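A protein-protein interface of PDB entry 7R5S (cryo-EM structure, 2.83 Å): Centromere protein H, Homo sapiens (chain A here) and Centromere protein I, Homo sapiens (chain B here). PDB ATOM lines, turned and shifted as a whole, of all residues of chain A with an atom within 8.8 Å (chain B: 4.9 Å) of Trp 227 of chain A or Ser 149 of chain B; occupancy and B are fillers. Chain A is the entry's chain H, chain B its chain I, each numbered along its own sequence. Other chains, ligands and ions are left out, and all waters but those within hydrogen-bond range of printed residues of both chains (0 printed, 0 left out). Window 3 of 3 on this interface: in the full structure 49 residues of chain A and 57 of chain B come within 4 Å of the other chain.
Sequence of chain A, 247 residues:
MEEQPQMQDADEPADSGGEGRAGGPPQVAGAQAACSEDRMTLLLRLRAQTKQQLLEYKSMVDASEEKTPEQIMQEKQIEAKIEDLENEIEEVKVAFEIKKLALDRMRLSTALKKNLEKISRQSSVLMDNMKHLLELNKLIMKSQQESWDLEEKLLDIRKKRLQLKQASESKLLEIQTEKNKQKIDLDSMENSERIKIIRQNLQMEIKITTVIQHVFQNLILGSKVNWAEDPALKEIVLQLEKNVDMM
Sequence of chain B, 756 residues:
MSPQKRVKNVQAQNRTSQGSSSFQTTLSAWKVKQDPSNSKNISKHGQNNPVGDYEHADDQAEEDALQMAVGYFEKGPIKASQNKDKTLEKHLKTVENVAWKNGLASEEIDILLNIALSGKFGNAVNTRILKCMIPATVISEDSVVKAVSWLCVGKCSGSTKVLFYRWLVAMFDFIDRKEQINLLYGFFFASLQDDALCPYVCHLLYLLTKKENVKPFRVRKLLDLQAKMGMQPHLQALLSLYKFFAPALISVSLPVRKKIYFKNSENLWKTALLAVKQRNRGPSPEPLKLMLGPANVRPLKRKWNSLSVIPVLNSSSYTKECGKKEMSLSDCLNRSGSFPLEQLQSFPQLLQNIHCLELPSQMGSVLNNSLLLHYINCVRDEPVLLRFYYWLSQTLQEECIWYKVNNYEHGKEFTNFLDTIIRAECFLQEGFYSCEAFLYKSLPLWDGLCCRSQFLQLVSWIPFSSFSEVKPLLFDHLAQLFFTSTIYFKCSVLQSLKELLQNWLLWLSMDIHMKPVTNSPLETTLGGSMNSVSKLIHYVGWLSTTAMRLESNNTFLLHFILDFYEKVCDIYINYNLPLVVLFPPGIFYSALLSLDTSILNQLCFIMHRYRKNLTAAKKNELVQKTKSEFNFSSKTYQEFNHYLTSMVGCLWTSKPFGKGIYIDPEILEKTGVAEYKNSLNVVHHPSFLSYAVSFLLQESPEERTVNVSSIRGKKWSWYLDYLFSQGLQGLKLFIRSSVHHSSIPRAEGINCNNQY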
ATOM      1  N   GLN A 217      14.175  10.634 -23.962  1.00  0.00           N
ATOM      2  CA  GLN A 217      13.549   9.335 -23.733  1.00  0.00           C
ATOM      3  C   GLN A 217      13.845   8.827 -22.327  1.00  0.00           C
ATOM      4  O   GLN A 217      12.941   8.371 -21.615  1.00  0.00           O
ATOM      5  CB  GLN A 217      14.023   8.328 -24.781  1.00  0.00           C
ATOM      6  CG  GLN A 217      13.358   6.966 -24.667  1.00  0.00           C
ATOM      7  CD  GLN A 217      13.933   5.954 -25.637  1.00  0.00           C
ATOM      8  OE1 GLN A 217      15.029   6.137 -26.164  1.00  0.00           O
ATOM      9  NE2 GLN A 217      13.191   4.881 -25.879  1.00  0.00           N
ATOM     10  N   LEU A 219      14.685  10.588 -19.704  1.00  0.00           N
ATOM     11  CA  LEU A 219      14.020  11.439 -18.722  1.00  0.00           C
ATOM     12  C   LEU A 219      12.540  11.098 -18.604  1.00  0.00           C
ATOM     13  O   LEU A 219      12.005  11.008 -17.492  1.00  0.00           O
ATOM     14  CB  LEU A 219      14.200  12.910 -19.091  1.00  0.00           C
ATOM     15  CG  LEU A 219      15.370  13.643 -18.433  1.00  0.00           C
ATOM     16  CD1 LEU A 219      15.369  15.106 -18.842  1.00  0.00           C
ATOM     17  CD2 LEU A 219      15.307  13.505 -16.921  1.00  0.00           C
ATOM     18  N   ILE A 220      11.860  10.913 -19.738  1.00  0.00           N
ATOM     19  CA  ILE A 220      10.442  10.562 -19.704  1.00  0.00           C
ATOM     20  C   ILE A 220      10.248   9.201 -19.050  1.00  0.00           C
ATOM     21  O   ILE A 220       9.267   8.974 -18.330  1.00  0.00           O
ATOM     22  CB  ILE A 220       9.848  10.607 -21.125  1.00  0.00           C
ATOM     23  CG1 ILE A 220       9.842  12.044 -21.648  1.00  0.00           C
ATOM     24  CG2 ILE A 220       8.440  10.034 -21.145  1.00  0.00           C
ATOM     25  CD1 ILE A 220       9.245  12.191 -23.027  1.00  0.00           C
ATOM     26  N   LEU A 221      11.187   8.278 -19.271  1.00  0.00           N
ATOM     27  CA  LEU A 221      11.098   6.969 -18.631  1.00  0.00           C
ATOM     28  C   LEU A 221      11.270   7.079 -17.120  1.00  0.00           C
ATOM     29  O   LEU A 221      10.496   6.494 -16.353  1.00  0.00           O
ATOM     30  CB  LEU A 221      12.146   6.027 -19.222  1.00  0.00           C
ATOM     31  CG  LEU A 221      12.384   4.736 -18.436  1.00  0.00           C
ATOM     32  CD1 LEU A 221      11.333   3.690 -18.776  1.00  0.00           C
ATOM     33  CD2 LEU A 221      13.784   4.211 -18.690  1.00  0.00           C
ATOM     34  N   GLY A 222      12.282   7.827 -16.673  1.00  0.00           N
ATOM     35  CA  GLY A 222      12.573   7.916 -15.253  1.00  0.00           C
ATOM     36  C   GLY A 222      11.647   8.813 -14.465  1.00  0.00           C
ATOM     37  O   GLY A 222      11.603   8.708 -13.236  1.00  0.00           O
ATOM     38  N   SER A 223      10.906   9.695 -15.139  1.00  0.00           N
ATOM     39  CA  SER A 223       9.991  10.584 -14.433  1.00  0.00           C
ATOM     40  C   SER A 223       8.763   9.862 -13.893  1.00  0.00           C
ATOM     41  O   SER A 223       8.071  10.423 -13.036  1.00  0.00           O
ATOM     42  CB  SER A 223       9.555  11.725 -15.352  1.00  0.00           C
ATOM     43  OG  SER A 223       8.430  11.353 -16.127  1.00  0.00           O
ATOM     44  N   LYS A 224       8.484   8.646 -14.365  1.00  0.00           N
ATOM     45  CA  LYS A 224       7.348   7.844 -13.912  1.00  0.00           C
ATOM     46  C   LYS A 224       6.031   8.603 -14.085  1.00  0.00           C
ATOM     47  O   LYS A 224       5.294   8.860 -13.130  1.00  0.00           O
ATOM     48  CB  LYS A 224       7.540   7.390 -12.461  1.00  0.00           C
ATOM     49  CG  LYS A 224       8.507   6.229 -12.297  1.00  0.00           C
ATOM     50  CD  LYS A 224       8.431   5.643 -10.896  1.00  0.00           C
ATOM     51  CE  LYS A 224       9.321   4.419 -10.762  1.00  0.00           C
ATOM     52  NZ  LYS A 224       9.197   3.787  -9.418  1.00  0.00           N
ATOM     53  N   VAL A 225       5.745   8.959 -15.335  1.00  0.00           N
ATOM     54  CA  VAL A 225       4.522   9.665 -15.691  1.00  0.00           C
ATOM     55  C   VAL A 225       3.812   8.879 -16.785  1.00  0.00           C
ATOM     56  O   VAL A 225       4.441   8.162 -17.570  1.00  0.00           O
ATOM     57  CB  VAL A 225       4.806  11.117 -16.144  1.00  0.00           C
ATOM     58  CG1 VAL A 225       5.497  11.137 -17.501  1.00  0.00           C
ATOM     59  CG2 VAL A 225       3.527  11.944 -16.164  1.00  0.00           C
ATOM     60  N   ASN A 226       2.488   9.004 -16.821  1.00  0.00           N
ATOM     61  CA  ASN A 226       1.668   8.336 -17.827  1.00  0.00           C
ATOM     62  C   ASN A 226       1.563   9.246 -19.046  1.00  0.00           C
ATOM     63  O   ASN A 226       0.879  10.274 -19.005  1.00  0.00           O
ATOM     64  CB  ASN A 226       0.289   8.004 -17.264  1.00  0.00           C
ATOM     65  CG  ASN A 226      -0.370   6.845 -17.983  1.00  0.00           C
ATOM     66  OD1 ASN A 226      -0.073   6.570 -19.145  1.00  0.00           O
ATOM     67  ND2 ASN A 226      -1.274   6.158 -17.294  1.00  0.00           N
ATOM     68  N   TRP A 227       2.239   8.867 -20.130  1.00  0.00           N
ATOM     69  CA  TRP A 227       2.268   9.687 -21.334  1.00  0.00           C
ATOM     70  C   TRP A 227       1.169   9.338 -22.328  1.00  0.00           C
ATOM     71  O   TRP A 227       0.899  10.137 -23.232  1.00  0.00           O
ATOM     72  CB  TRP A 227       3.631   9.564 -22.025  1.00  0.00           C
ATOM     73  CG  TRP A 227       4.204   8.180 -21.998  1.00  0.00           C
ATOM     74  CD1 TRP A 227       5.068   7.669 -21.076  1.00  0.00           C
ATOM     75  CD2 TRP A 227       3.961   7.133 -22.944  1.00  0.00           C
ATOM     76  NE1 TRP A 227       5.375   6.366 -21.385  1.00  0.00           N
ATOM     77  CE2 TRP A 227       4.708   6.012 -22.528  1.00  0.00           C
ATOM     78  CE3 TRP A 227       3.181   7.030 -24.100  1.00  0.00           C
ATOM     79  CZ2 TRP A 227       4.699   4.808 -23.227  1.00  0.00           C
ATOM     80  CZ3 TRP A 227       3.175   5.834 -24.793  1.00  0.00           C
ATOM     81  CH2 TRP A 227       3.928   4.739 -24.354  1.00  0.00           C
ATOM     82  N   ALA A 228       0.533   8.174 -22.188  1.00  0.00           N
ATOM     83  CA  ALA A 228      -0.522   7.790 -23.118  1.00  0.00           C
ATOM     84  C   ALA A 228      -1.773   8.645 -22.967  1.00  0.00           C
ATOM     85  O   ALA A 228      -2.540   8.773 -23.927  1.00  0.00           O
ATOM     86  CB  ALA A 228      -0.877   6.314 -22.933  1.00  0.00           C
ATOM     87  N   GLU A 229      -1.997   9.232 -21.789  1.00  0.00           N
ATOM     88  CA  GLU A 229      -3.176  10.070 -21.596  1.00  0.00           C
ATOM     89  C   GLU A 229      -3.037  11.414 -22.299  1.00  0.00           C
ATOM     90  O   GLU A 229      -4.032  11.956 -22.794  1.00  0.00           O
ATOM     91  CB  GLU A 229      -3.436  10.274 -20.103  1.00  0.00           C
ATOM     92  CG  GLU A 229      -4.425   9.285 -19.499  1.00  0.00           C
ATOM     93  CD  GLU A 229      -4.034   7.840 -19.738  1.00  0.00           C
ATOM     94  OE1 GLU A 229      -2.830   7.521 -19.644  1.00  0.00           O
ATOM     95  OE2 GLU A 229      -4.932   7.019 -20.019  1.00  0.00           O
ATOM     96  N   ASP A 230      -1.825  11.965 -22.356  1.00  0.00           N
ATOM     97  CA  ASP A 230      -1.596  13.243 -23.010  1.00  0.00           C
ATOM     98  C   ASP A 230      -1.107  13.002 -24.428  1.00  0.00           C
ATOM     99  O   ASP A 230       0.021  12.518 -24.608  1.00  0.00           O
ATOM    100  CB  ASP A 230      -0.580  14.075 -22.229  1.00  0.00           C
ATOM    101  CG  ASP A 230      -0.356  15.443 -22.839  1.00  0.00           C
ATOM    102  OD1 ASP A 230      -1.283  16.277 -22.791  1.00  0.00           O
ATOM    103  OD2 ASP A 230       0.751  15.687 -23.367  1.00  0.00           O
ATOM    104  N   PRO A 231      -1.900  13.309 -25.458  1.00  0.00           N
ATOM    105  CA  PRO A 231      -1.435  13.061 -26.832  1.00  0.00           C
ATOM    106  C   PRO A 231      -0.272  13.943 -27.245  1.00  0.00           C
ATOM    107  O   PRO A 231       0.541  13.524 -28.079  1.00  0.00           O
ATOM    108  CB  PRO A 231      -2.684  13.338 -27.684  1.00  0.00           C
ATOM    109  CG  PRO A 231      -3.837  13.299 -26.722  1.00  0.00           C
ATOM    110  CD  PRO A 231      -3.289  13.793 -25.422  1.00  0.00           C
ATOM    111  N   ALA A 232      -0.169  15.155 -26.692  1.00  0.00           N
ATOM    112  CA  ALA A 232       0.933  16.043 -27.048  1.00  0.00           C
ATOM    113  C   ALA A 232       2.278  15.417 -26.702  1.00  0.00           C
ATOM    114  O   ALA A 232       3.252  15.561 -27.452  1.00  0.00           O
ATOM    115  CB  ALA A 232       0.770  17.392 -26.348  1.00  0.00           C
ATOM    116  N   LEU A 233       2.353  14.718 -25.569  1.00  0.00           N
ATOM    117  CA  LEU A 233       3.567  13.991 -25.220  1.00  0.00           C
ATOM    118  C   LEU A 233       3.635  12.643 -25.927  1.00  0.00           C
ATOM    119  O   LEU A 233       4.732  12.110 -26.133  1.00  0.00           O
ATOM    120  CB  LEU A 233       3.646  13.803 -23.704  1.00  0.00           C
ATOM    121  CG  LEU A 233       4.979  13.327 -23.123  1.00  0.00           C
ATOM    122  CD1 LEU A 233       6.074  14.343 -23.396  1.00  0.00           C
ATOM    123  CD2 LEU A 233       4.846  13.066 -21.631  1.00  0.00           C
ATOM    124  N   LYS A 234       2.483  12.085 -26.305  1.00  0.00           N
ATOM    125  CA  LYS A 234       2.475  10.807 -27.009  1.00  0.00           C
ATOM    126  C   LYS A 234       3.119  10.934 -28.384  1.00  0.00           C
ATOM    127  O   LYS A 234       3.874  10.050 -28.807  1.00  0.00           O
ATOM    128  CB  LYS A 234       1.044  10.283 -27.131  1.00  0.00           C
ATOM    129  CG  LYS A 234       0.946   8.865 -27.665  1.00  0.00           C
ATOM    130  CD  LYS A 234      -0.482   8.350 -27.598  1.00  0.00           C
ATOM    131  CE  LYS A 234      -0.572   6.902 -28.052  1.00  0.00           C
ATOM    132  NZ  LYS A 234      -1.958   6.370 -27.942  1.00  0.00           N
ATOM    133  N   GLU A 235       2.835  12.026 -29.095  1.00  0.00           N
ATOM    134  CA  GLU A 235       3.479  12.250 -30.386  1.00  0.00           C
ATOM    135  C   GLU A 235       4.993  12.321 -30.234  1.00  0.00           C
ATOM    136  O   GLU A 235       5.740  11.768 -31.050  1.00  0.00           O
ATOM    137  CB  GLU A 235       2.938  13.528 -31.036  1.00  0.00           C
ATOM    138  CG  GLU A 235       1.410  13.663 -31.082  1.00  0.00           C
ATOM    139  CD  GLU A 235       0.686  12.475 -31.706  1.00  0.00           C
ATOM    140  OE1 GLU A 235       1.326  11.646 -32.388  1.00  0.00           O
ATOM    141  OE2 GLU A 235      -0.543  12.371 -31.511  1.00  0.00           O
ATOM    142  N   ILE A 236       5.464  12.979 -29.174  1.00  0.00           N
ATOM    143  CA  ILE A 236       6.903  13.109 -28.956  1.00  0.00           C
ATOM    144  C   ILE A 236       7.524  11.751 -28.650  1.00  0.00           C
ATOM    145  O   ILE A 236       8.549  11.375 -29.230  1.00  0.00           O
ATOM    146  CB  ILE A 236       7.185  14.126 -27.835  1.00  0.00           C
ATOM    147  CG1 ILE A 236       6.627  15.500 -28.211  1.00  0.00           C
ATOM    148  CG2 ILE A 236       8.677  14.210 -27.557  1.00  0.00           C
ATOM    149  CD1 ILE A 236       7.220  16.073 -29.479  1.00  0.00           C
ATOM    150  N   VAL A 237       6.912  10.992 -27.736  1.00  0.00           N
ATOM    151  CA  VAL A 237       7.478   9.698 -27.370  1.00  0.00           C
ATOM    152  C   VAL A 237       7.368   8.690 -28.506  1.00  0.00           C
ATOM    153  O   VAL A 237       8.097   7.691 -28.512  1.00  0.00           O
ATOM    154  CB  VAL A 237       6.827   9.140 -26.090  1.00  0.00           C
ATOM    155  CG1 VAL A 237       6.895  10.162 -24.967  1.00  0.00           C
ATOM    156  CG2 VAL A 237       5.394   8.717 -26.354  1.00  0.00           C
ATOM    157  N   LEU A 238       6.477   8.918 -29.472  1.00  0.00           N
ATOM    158  CA  LEU A 238       6.427   8.076 -30.658  1.00  0.00           C
ATOM    159  C   LEU A 238       7.407   8.515 -31.737  1.00  0.00           C
ATOM    160  O   LEU A 238       7.851   7.677 -32.529  1.00  0.00           O
ATOM    161  CB  LEU A 238       5.008   8.054 -31.236  1.00  0.00           C
ATOM    162  CG  LEU A 238       3.976   7.248 -30.444  1.00  0.00           C
ATOM    163  CD1 LEU A 238       2.603   7.353 -31.088  1.00  0.00           C
ATOM    164  CD2 LEU A 238       4.408   5.795 -30.329  1.00  0.00           C
ATOM    165  N   VAL B 145       0.141  -0.261 -26.530  1.00  0.00           N
ATOM    166  CA  VAL B 145       0.832   0.971 -26.157  1.00  0.00           C
ATOM    167  C   VAL B 145       0.340   1.471 -24.804  1.00  0.00           C
ATOM    168  O   VAL B 145       1.136   1.870 -23.942  1.00  0.00           O
ATOM    169  CB  VAL B 145       0.657   2.037 -27.254  1.00  0.00           C
ATOM    170  CG1 VAL B 145       1.216   3.373 -26.793  1.00  0.00           C
ATOM    171  CG2 VAL B 145       1.340   1.591 -28.537  1.00  0.00           C
ATOM    172  N   LYS B 146      -0.979   1.454 -24.592  1.00  0.00           N
ATOM    173  CA  LYS B 146      -1.526   1.868 -23.305  1.00  0.00           C
ATOM    174  C   LYS B 146      -1.079   0.932 -22.189  1.00  0.00           C
ATOM    175  O   LYS B 146      -0.826   1.373 -21.062  1.00  0.00           O
ATOM    176  CB  LYS B 146      -3.052   1.930 -23.376  1.00  0.00           C
ATOM    177  CG  LYS B 146      -3.588   3.064 -24.232  1.00  0.00           C
ATOM    178  CD  LYS B 146      -5.108   3.075 -24.240  1.00  0.00           C
ATOM    179  CE  LYS B 146      -5.647   4.260 -25.022  1.00  0.00           C
ATOM    180  NZ  LYS B 146      -7.133   4.241 -25.100  1.00  0.00           N
ATOM    181  N   ALA B 147      -0.972  -0.365 -22.486  1.00  0.00           N
ATOM    182  CA  ALA B 147      -0.493  -1.314 -21.485  1.00  0.00           C
ATOM    183  C   ALA B 147       0.960  -1.038 -21.114  1.00  0.00           C
ATOM    184  O   ALA B 147       1.332  -1.103 -19.937  1.00  0.00           O
ATOM    185  CB  ALA B 147      -0.656  -2.743 -22.001  1.00  0.00           C
ATOM    186  N   VAL B 148       1.795  -0.727 -22.108  1.00  0.00           N
ATOM    187  CA  VAL B 148       3.190  -0.398 -21.832  1.00  0.00           C
ATOM    188  C   VAL B 148       3.282   0.882 -21.010  1.00  0.00           C
ATOM    189  O   VAL B 148       4.106   0.992 -20.094  1.00  0.00           O
ATOM    190  CB  VAL B 148       3.981  -0.292 -23.148  1.00  0.00           C
ATOM    191  CG1 VAL B 148       5.358   0.307 -22.902  1.00  0.00           C
ATOM    192  CG2 VAL B 148       4.105  -1.657 -23.800  1.00  0.00           C
ATOM    193  N   SER B 149       2.433   1.867 -21.314  1.00  0.00           N
ATOM    194  CA  SER B 149       2.418   3.090 -20.518  1.00  0.00           C
ATOM    195  C   SER B 149       1.994   2.819 -19.079  1.00  0.00           C
ATOM    196  O   SER B 149       2.585   3.371 -18.142  1.00  0.00           O
ATOM    197  CB  SER B 149       1.491   4.123 -21.159  1.00  0.00           C
ATOM    198  OG  SER B 149       1.361   5.269 -20.337  1.00  0.00           O
ATOM    199  N   TRP B 150       0.982   1.970 -18.882  1.00  0.00           N
ATOM    200  CA  TRP B 150       0.547   1.639 -17.529  1.00  0.00           C
ATOM    201  C   TRP B 150       1.626   0.870 -16.776  1.00  0.00           C
ATOM    202  O   TRP B 150       1.763   1.018 -15.556  1.00  0.00           O
ATOM    203  CB  TRP B 150      -0.754   0.838 -17.572  1.00  0.00           C
ATOM    204  CG  TRP B 150      -1.982   1.691 -17.667  1.00  0.00           C
ATOM    205  CD1 TRP B 150      -2.850   1.764 -18.716  1.00  0.00           C
ATOM    206  CD2 TRP B 150      -2.475   2.600 -16.675  1.00  0.00           C
ATOM    207  NE1 TRP B 150      -3.856   2.658 -18.437  1.00  0.00           N
ATOM    208  CE2 TRP B 150      -3.647   3.186 -17.190  1.00  0.00           C
ATOM    209  CE3 TRP B 150      -2.039   2.974 -15.400  1.00  0.00           C
ATOM    210  CZ2 TRP B 150      -4.389   4.124 -16.476  1.00  0.00           C
ATOM    211  CZ3 TRP B 150      -2.776   3.906 -14.693  1.00  0.00           C
ATOM    212  CH2 TRP B 150      -3.938   4.469 -15.233  1.00  0.00           C
ATOM    213  N   LEU B 151       2.393   0.038 -17.484  1.00  0.00           N
ATOM    214  CA  LEU B 151       3.540  -0.611 -16.858  1.00  0.00           C
ATOM    215  C   LEU B 151       4.594   0.411 -16.456  1.00  0.00           C
ATOM    216  O   LEU B 151       5.182   0.317 -15.373  1.00  0.00           O
ATOM    217  CB  LEU B 151       4.144  -1.649 -17.804  1.00  0.00           C
ATOM    218  CG  LEU B 151       3.521  -3.043 -17.814  1.00  0.00           C
ATOM    219  CD1 LEU B 151       4.470  -4.024 -18.478  1.00  0.00           C
ATOM    220  CD2 LEU B 151       3.180  -3.492 -16.403  1.00  0.00           C
ATOM    221  N   CYS B 152       4.845   1.395 -17.319  1.00  0.00           N
ATOM    222  CA  CYS B 152       5.798   2.453 -17.009  1.00  0.00           C
ATOM    223  C   CYS B 152       5.315   3.369 -15.894  1.00  0.00           C
ATOM    224  O   CYS B 152       6.132   4.095 -15.318  1.00  0.00           O
ATOM    225  CB  CYS B 152       6.094   3.277 -18.263  1.00  0.00           C
ATOM    226  SG  CYS B 152       7.398   2.589 -19.308  1.00  0.00           S
ATOM    227  N   VAL B 153       4.017   3.361 -15.585  1.00  0.00           N
ATOM    228  CA  VAL B 153       3.519   4.145 -14.456  1.00  0.00           C
ATOM    229  C   VAL B 153       4.128   3.642 -13.152  1.00  0.00           C
ATOM    230  O   VAL B 153       4.618   4.429 -12.332  1.00  0.00           O
ATOM    231  CB  VAL B 153       1.981   4.108 -14.412  1.00  0.00           C
ATOM    232  CG1 VAL B 153       1.475   4.622 -13.074  1.00  0.00           C
ATOM    233  CG2 VAL B 153       1.400   4.927 -15.552  1.00  0.00           C
ATOM    234  N   LEU B 184       8.874   1.218 -29.570  1.00  0.00           N
ATOM    235  CA  LEU B 184       8.992   1.291 -28.118  1.00  0.00           C
ATOM    236  C   LEU B 184      10.069   0.340 -27.606  1.00  0.00           C
ATOM    237  O   LEU B 184       9.894  -0.341 -26.593  1.00  0.00           O
ATOM    238  CB  LEU B 184       7.652   0.993 -27.450  1.00  0.00           C
ATOM    239  CG  LEU B 184       6.512   1.970 -27.739  1.00  0.00           C
ATOM    240  CD1 LEU B 184       5.231   1.516 -27.061  1.00  0.00           C
ATOM    241  CD2 LEU B 184       6.885   3.375 -27.296  1.00  0.00           C
ATOM    242  N   PHE B 187      11.794   1.352 -23.949  1.00  0.00           N
ATOM    243  CA  PHE B 187      11.041   1.043 -22.738  1.00  0.00           C
ATOM    244  C   PHE B 187      11.132  -0.434 -22.382  1.00  0.00           C
ATOM    245  O   PHE B 187      11.069  -0.790 -21.200  1.00  0.00           O
ATOM    246  CB  PHE B 187       9.582   1.464 -22.905  1.00  0.00           C
ATOM    247  CG  PHE B 187       9.397   2.942 -23.092  1.00  0.00           C
ATOM    248  CD1 PHE B 187       9.305   3.487 -24.361  1.00  0.00           C
ATOM    249  CD2 PHE B 187       9.320   3.788 -21.999  1.00  0.00           C
ATOM    250  CE1 PHE B 187       9.135   4.848 -24.536  1.00  0.00           C
ATOM    251  CE2 PHE B 187       9.151   5.149 -22.167  1.00  0.00           C
ATOM    252  CZ  PHE B 187       9.058   5.679 -23.437  1.00  0.00           C
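Among the printed residues, pairs that only touch across the chains: Asn 226 of chain A with Val 153 of chain B (3.4 Å), Ala 228 of chain A with Ser 149 of chain B (3.5 Å), Trp 227 of chain A with Ser 149 of chain B (3.7 Å), Trp 227 of chain A with Val 145 of chain B (3.7 Å), Asn 226 of chain A with Trp 150 of chain B (3.8 Å) and Leu 221 of chain A with Phe 187 of chain B (3.8 Å).
Hydrophobic or aromatic side chains of chain B that line the printed part of chain A: Val 145, Trp 150, Val 153 and Phe 187. Along chain B the printed residues that touch a printed residue of chain A span positions 145 to 187. Of the 21 printed residues of chain A, 4 touch a printed residue of chain B. Hydrophobic or aromatic side chains of chain A that line the printed part of chain B: Leu 221, Trp 227 and Ala 228. Among the printed residues, no Asp or Glu carboxylate lies within 4 Å of a Lys or Arg side-chain nitrogen of the other chain.
N of Ala 228 of chain A lies close to OD1 of Asn 226 of chain A (3.5 Å). The side-chain amide oxygen (OD1) of Asn 226 of chain A lies close to the side-chain carboxylate (OE1) of Glu 229 of chain A (3.0 Å).
OG of Ser 149 of chain B sits close to OD1 of Asn 226 of chain A.
Printed residues of chain B within 4 Å of Leu 221 of chain A: Phe 187 (3.8 Å). Of the printed residues of chain B, Trp 227 of chain A touches Val 145 (3.7 Å) and Ser 149 (3.7 Å). Lys 234 of chain A touches none of the printed residues of chain B. Printed residues of chain A within 4 Å of Val 145 of chain B: Trp 227. No residue of chain A comes within 4 Å of Val 148 of chain B. Of chain A, only Asn 226 (2.3 Å), Trp 227 (3.7 Å) and Ala 228 (3.5 Å) come within 4 Å of Ser 149 of chain B. Printed residues of chain A within 4 Å of Phe 187 of chain B: Leu 221 (3.8 Å). The nearest residue of chain B that does not touch Trp 227 of chain A is Phe 187 of chain B (4.04 Å). The nearest printed residue of chain B that does not touch Asn 226 of chain A is Lys 146 of chain B (5.6 Å).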
